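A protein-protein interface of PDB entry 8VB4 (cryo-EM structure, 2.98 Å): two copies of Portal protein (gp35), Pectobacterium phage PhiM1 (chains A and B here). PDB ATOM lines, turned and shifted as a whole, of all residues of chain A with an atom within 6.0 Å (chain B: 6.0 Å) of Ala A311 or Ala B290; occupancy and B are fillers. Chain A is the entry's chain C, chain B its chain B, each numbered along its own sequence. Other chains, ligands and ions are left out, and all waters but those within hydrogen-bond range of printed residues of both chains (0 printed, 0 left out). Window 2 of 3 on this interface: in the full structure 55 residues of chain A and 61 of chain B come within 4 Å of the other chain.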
ATOM      1  N   GLN A 295      16.083 -25.825 -34.411  1.00  0.00           N
ATOM      2  CA  GLN A 295      14.955 -26.528 -33.816  1.00  0.00           C
ATOM      3  C   GLN A 295      13.653 -25.819 -34.166  1.00  0.00           C
ATOM      4  O   GLN A 295      13.428 -24.677 -33.758  1.00  0.00           O
ATOM      5  CB  GLN A 295      15.121 -26.596 -32.299  1.00  0.00           C
ATOM      6  CG  GLN A 295      16.308 -27.423 -31.834  1.00  0.00           C
ATOM      7  CD  GLN A 295      16.124 -28.903 -32.096  1.00  0.00           C
ATOM      8  OE1 GLN A 295      15.027 -29.440 -31.948  1.00  0.00           O
ATOM      9  NE2 GLN A 295      17.202 -29.573 -32.487  1.00  0.00           N
ATOM     10  N   ILE A 296      12.790 -26.500 -34.921  1.00  0.00           N
ATOM     11  CA  ILE A 296      11.501 -25.942 -35.312  1.00  0.00           C
ATOM     12  C   ILE A 296      10.526 -27.090 -35.510  1.00  0.00           C
ATOM     13  O   ILE A 296      10.925 -28.249 -35.631  1.00  0.00           O
ATOM     14  CB  ILE A 296      11.618 -25.079 -36.595  1.00  0.00           C
ATOM     15  CG1 ILE A 296      12.457 -25.797 -37.651  1.00  0.00           C
ATOM     16  CG2 ILE A 296      12.228 -23.727 -36.274  1.00  0.00           C
ATOM     17  CD1 ILE A 296      12.358 -25.174 -39.022  1.00  0.00           C
ATOM     18  N   ASP A 297       9.236 -26.764 -35.539  1.00  0.00           N
ATOM     19  CA  ASP A 297       8.169 -27.727 -35.810  1.00  0.00           C
ATOM     20  C   ASP A 297       7.439 -27.239 -37.057  1.00  0.00           C
ATOM     21  O   ASP A 297       6.445 -26.518 -36.977  1.00  0.00           O
ATOM     22  CB  ASP A 297       7.236 -27.852 -34.612  1.00  0.00           C
ATOM     23  CG  ASP A 297       6.221 -28.963 -34.777  1.00  0.00           C
ATOM     24  OD1 ASP A 297       6.400 -29.804 -35.682  1.00  0.00           O
ATOM     25  OD2 ASP A 297       5.243 -28.996 -34.002  1.00  0.00           O
ATOM     26  N   TRP A 309      -0.047 -21.259 -30.235  1.00  0.00           N
ATOM     27  CA  TRP A 309       1.288 -21.264 -29.658  1.00  0.00           C
ATOM     28  C   TRP A 309       2.026 -22.523 -30.090  1.00  0.00           C
ATOM     29  O   TRP A 309       1.476 -23.628 -30.054  1.00  0.00           O
ATOM     30  CB  TRP A 309       1.239 -21.194 -28.127  1.00  0.00           C
ATOM     31  CG  TRP A 309       0.788 -19.869 -27.588  1.00  0.00           C
ATOM     32  CD1 TRP A 309      -0.079 -18.996 -28.175  1.00  0.00           C
ATOM     33  CD2 TRP A 309       1.197 -19.261 -26.358  1.00  0.00           C
ATOM     34  NE1 TRP A 309      -0.241 -17.886 -27.385  1.00  0.00           N
ATOM     35  CE2 TRP A 309       0.533 -18.024 -26.264  1.00  0.00           C
ATOM     36  CE3 TRP A 309       2.058 -19.644 -25.328  1.00  0.00           C
ATOM     37  CZ2 TRP A 309       0.703 -17.168 -25.181  1.00  0.00           C
ATOM     38  CZ3 TRP A 309       2.225 -18.793 -24.253  1.00  0.00           C
ATOM     39  CH2 TRP A 309       1.552 -17.570 -24.188  1.00  0.00           C
ATOM     40  N   VAL A 310       3.282 -22.348 -30.500  1.00  0.00           N
ATOM     41  CA  VAL A 310       4.094 -23.434 -31.035  1.00  0.00           C
ATOM     42  C   VAL A 310       5.462 -23.378 -30.369  1.00  0.00           C
ATOM     43  O   VAL A 310       5.872 -22.347 -29.833  1.00  0.00           O
ATOM     44  CB  VAL A 310       4.218 -23.340 -32.576  1.00  0.00           C
ATOM     45  CG1 VAL A 310       5.093 -24.456 -33.126  1.00  0.00           C
ATOM     46  CG2 VAL A 310       2.839 -23.374 -33.218  1.00  0.00           C
ATOM     47  N   ALA A 311       6.168 -24.504 -30.399  1.00  0.00           N
ATOM     48  CA  ALA A 311       7.493 -24.623 -29.805  1.00  0.00           C
ATOM     49  C   ALA A 311       8.542 -24.639 -30.906  1.00  0.00           C
ATOM     50  O   ALA A 311       8.480 -25.470 -31.817  1.00  0.00           O
ATOM     51  CB  ALA A 311       7.601 -25.891 -28.957  1.00  0.00           C
ATOM     52  N   GLY A 312       9.496 -23.732 -30.817  1.00  0.00           N
ATOM     53  CA  GLY A 312      10.569 -23.634 -31.787  1.00  0.00           C
ATOM     54  C   GLY A 312      11.173 -22.244 -31.778  1.00  0.00           C
ATOM     55  O   GLY A 312      10.648 -21.302 -31.194  1.00  0.00           O
ATOM     56  N   ASP A 313      12.312 -22.114 -32.445  1.00  0.00           N
ATOM     57  CA  ASP A 313      12.980 -20.825 -32.515  1.00  0.00           C
ATOM     58  C   ASP A 313      12.112 -19.837 -33.291  1.00  0.00           C
ATOM     59  O   ASP A 313      11.498 -20.208 -34.297  1.00  0.00           O
ATOM     60  CB  ASP A 313      14.345 -20.966 -33.190  1.00  0.00           C
ATOM     61  N   HIS B 288       3.051 -17.407 -31.865  1.00  0.00           N
ATOM     62  CA  HIS B 288       3.963 -17.122 -30.763  1.00  0.00           C
ATOM     63  C   HIS B 288       4.797 -18.368 -30.512  1.00  0.00           C
ATOM     64  O   HIS B 288       4.245 -19.457 -30.328  1.00  0.00           O
ATOM     65  CB  HIS B 288       3.202 -16.712 -29.500  1.00  0.00           C
ATOM     66  CG  HIS B 288       2.745 -15.288 -29.511  1.00  0.00           C
ATOM     67  ND1 HIS B 288       3.533 -14.249 -29.068  1.00  0.00           N
ATOM     68  CD2 HIS B 288       1.580 -14.730 -29.918  1.00  0.00           C
ATOM     69  CE1 HIS B 288       2.875 -13.112 -29.198  1.00  0.00           C
ATOM     70  NE2 HIS B 288       1.686 -13.376 -29.712  1.00  0.00           N
ATOM     71  N   MET B 289       6.115 -18.208 -30.502  1.00  0.00           N
ATOM     72  CA  MET B 289       7.037 -19.329 -30.408  1.00  0.00           C
ATOM     73  C   MET B 289       7.700 -19.355 -29.039  1.00  0.00           C
ATOM     74  O   MET B 289       8.232 -18.344 -28.574  1.00  0.00           O
ATOM     75  CB  MET B 289       8.104 -19.240 -31.500  1.00  0.00           C
ATOM     76  CG  MET B 289       7.547 -19.322 -32.910  1.00  0.00           C
ATOM     77  SD  MET B 289       7.102 -21.000 -33.387  1.00  0.00           S
ATOM     78  CE  MET B 289       7.052 -20.835 -35.168  1.00  0.00           C
ATOM     79  N   ALA B 290       7.669 -20.521 -28.399  1.00  0.00           N
ATOM     80  CA  ALA B 290       8.335 -20.728 -27.122  1.00  0.00           C
ATOM     81  C   ALA B 290       9.752 -21.225 -27.381  1.00  0.00           C
ATOM     82  O   ALA B 290       9.939 -22.326 -27.908  1.00  0.00           O
ATOM     83  CB  ALA B 290       7.562 -21.724 -26.263  1.00  0.00           C
ATOM     84  N   LYS B 291      10.742 -20.419 -27.007  1.00  0.00           N
ATOM     85  CA  LYS B 291      12.123 -20.766 -27.287  1.00  0.00           C
ATOM     86  C   LYS B 291      12.497 -22.069 -26.582  1.00  0.00           C
ATOM     87  O   LYS B 291      12.095 -22.303 -25.440  1.00  0.00           O
ATOM     88  CB  LYS B 291      13.058 -19.654 -26.827  1.00  0.00           C
ATOM     89  CG  LYS B 291      12.972 -18.383 -27.648  1.00  0.00           C
ATOM     90  CD  LYS B 291      13.825 -17.284 -27.039  1.00  0.00           C
ATOM     91  CE  LYS B 291      13.651 -15.971 -27.778  1.00  0.00           C
ATOM     92  NZ  LYS B 291      13.983 -14.802 -26.921  1.00  0.00           N
ATOM     93  N   PRO B 292      13.269 -22.937 -27.240  1.00  0.00           N
ATOM     94  CA  PRO B 292      13.751 -24.147 -26.567  1.00  0.00           C
ATOM     95  C   PRO B 292      15.012 -23.883 -25.761  1.00  0.00           C
ATOM     96  O   PRO B 292      15.890 -23.117 -26.159  1.00  0.00           O
ATOM     97  CB  PRO B 292      14.028 -25.097 -27.738  1.00  0.00           C
ATOM     98  CG  PRO B 292      14.438 -24.195 -28.843  1.00  0.00           C
ATOM     99  CD  PRO B 292      13.692 -22.895 -28.651  1.00  0.00           C
ATOM    100  N   ILE B 296      10.777 -21.536 -18.322  1.00  0.00           N
ATOM    101  CA  ILE B 296       9.501 -20.832 -18.353  1.00  0.00           C
ATOM    102  C   ILE B 296       8.429 -21.767 -17.819  1.00  0.00           C
ATOM    103  O   ILE B 296       8.630 -22.979 -17.725  1.00  0.00           O
ATOM    104  CB  ILE B 296       9.154 -20.341 -19.782  1.00  0.00           C
ATOM    105  CG1 ILE B 296       9.406 -21.447 -20.806  1.00  0.00           C
ATOM    106  CG2 ILE B 296       9.966 -19.108 -20.133  1.00  0.00           C
ATOM    107  CD1 ILE B 296       8.806 -21.160 -22.161  1.00  0.00           C
ATOM    108  N   VAL B 298       4.903 -22.407 -19.069  1.00  0.00           N
ATOM    109  CA  VAL B 298       4.006 -22.060 -20.167  1.00  0.00           C
ATOM    110  C   VAL B 298       2.554 -22.070 -19.705  1.00  0.00           C
ATOM    111  O   VAL B 298       1.764 -21.195 -20.081  1.00  0.00           O
ATOM    112  CB  VAL B 298       4.225 -23.010 -21.358  1.00  0.00           C
ATOM    113  CG1 VAL B 298       3.533 -22.472 -22.597  1.00  0.00           C
ATOM    114  CG2 VAL B 298       5.710 -23.199 -21.625  1.00  0.00           C
ATOM    115  N   GLY B 316      11.146 -15.578 -22.745  1.00  0.00           N
ATOM    116  CA  GLY B 316      11.125 -16.938 -23.251  1.00  0.00           C
ATOM    117  C   GLY B 316      10.180 -17.157 -24.413  1.00  0.00           C
ATOM    118  O   GLY B 316      10.273 -18.188 -25.085  1.00  0.00           O
ATOM    119  N   VAL B 317       9.274 -16.216 -24.666  1.00  0.00           N
ATOM    120  CA  VAL B 317       8.298 -16.322 -25.743  1.00  0.00           C
ATOM    121  C   VAL B 317       8.436 -15.102 -26.642  1.00  0.00           C
ATOM    122  O   VAL B 317       8.497 -13.968 -26.158  1.00  0.00           O
ATOM    123  CB  VAL B 317       6.860 -16.438 -25.197  1.00  0.00           C
ATOM    124  CG1 VAL B 317       5.848 -16.330 -26.326  1.00  0.00           C
ATOM    125  CG2 VAL B 317       6.685 -17.746 -24.445  1.00  0.00           C
ATOM    126  N   ALA B 318       8.483 -15.340 -27.952  1.00  0.00           N
ATOM    127  CA  ALA B 318       8.644 -14.273 -28.927  1.00  0.00           C
ATOM    128  C   ALA B 318       7.657 -14.474 -30.066  1.00  0.00           C
ATOM    129  O   ALA B 318       7.194 -15.587 -30.327  1.00  0.00           O
ATOM    130  CB  ALA B 318      10.076 -14.220 -29.472  1.00  0.00           C
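Ala A311 touches just one residue of chain B: Ala B290.
Ala B290 touches three residues of chain A.
Of the printed residues of chain B, Trp A309 touches His B288 (3.5 Å).
Printed residues of chain A within 4 Å of His B288: Trp A309 (3.5 Å) and Val A310 (3.1 Å).
Of the printed residues of chain A, Met B289 touches Val A310 and Gly A312.
Printed residues of chain B within 4 Å of Val A310: His B288, Met B289 and Ala B290.
Ile B296 touches none of the printed residues of chain A.
Hydrophobic or aromatic side chains of chain A that line the printed part of chain B: Val A310.
Along chain A the printed residues that touch a printed residue of chain B span positions 309 to 312.
Of the 10 printed residues of chain B, 3 touch a printed residue of chain A.
Hydrophobic or aromatic side chains of chain B within 4 Å of the printed part of chain A: Met B289 and Ala B290.
The backbone NH (N) of Met B289 sits at hydrogen-bond distance from the backbone carbonyl oxygen (O) of Ala B318, 2.8 Å away.
Position printed for both chains: 296.
Of the 7 pairs that touch across the chains among the printed residues, none has its exchanged pair printed and touching as well.
The backbone NH of Val A310 is in hydrogen-bond range of the backbone carbonyl oxygen of His B288 (3.1 Å).
N of Ala B290 is in hydrogen-bond range of O of Val A310 (2.9 Å).
The backbone carbonyl oxygen (O) of Ala B290 is in hydrogen-bond range of the backbone NH (N) of Gly A312 (3.3 Å).
O of His B288 touches CA of Trp A309, 3.5 Å away.
CA of Met B289 touches O of Val A310 (3.3 Å).
Ala A311 touches Ala B290.
Gly A312 touches Met B289.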
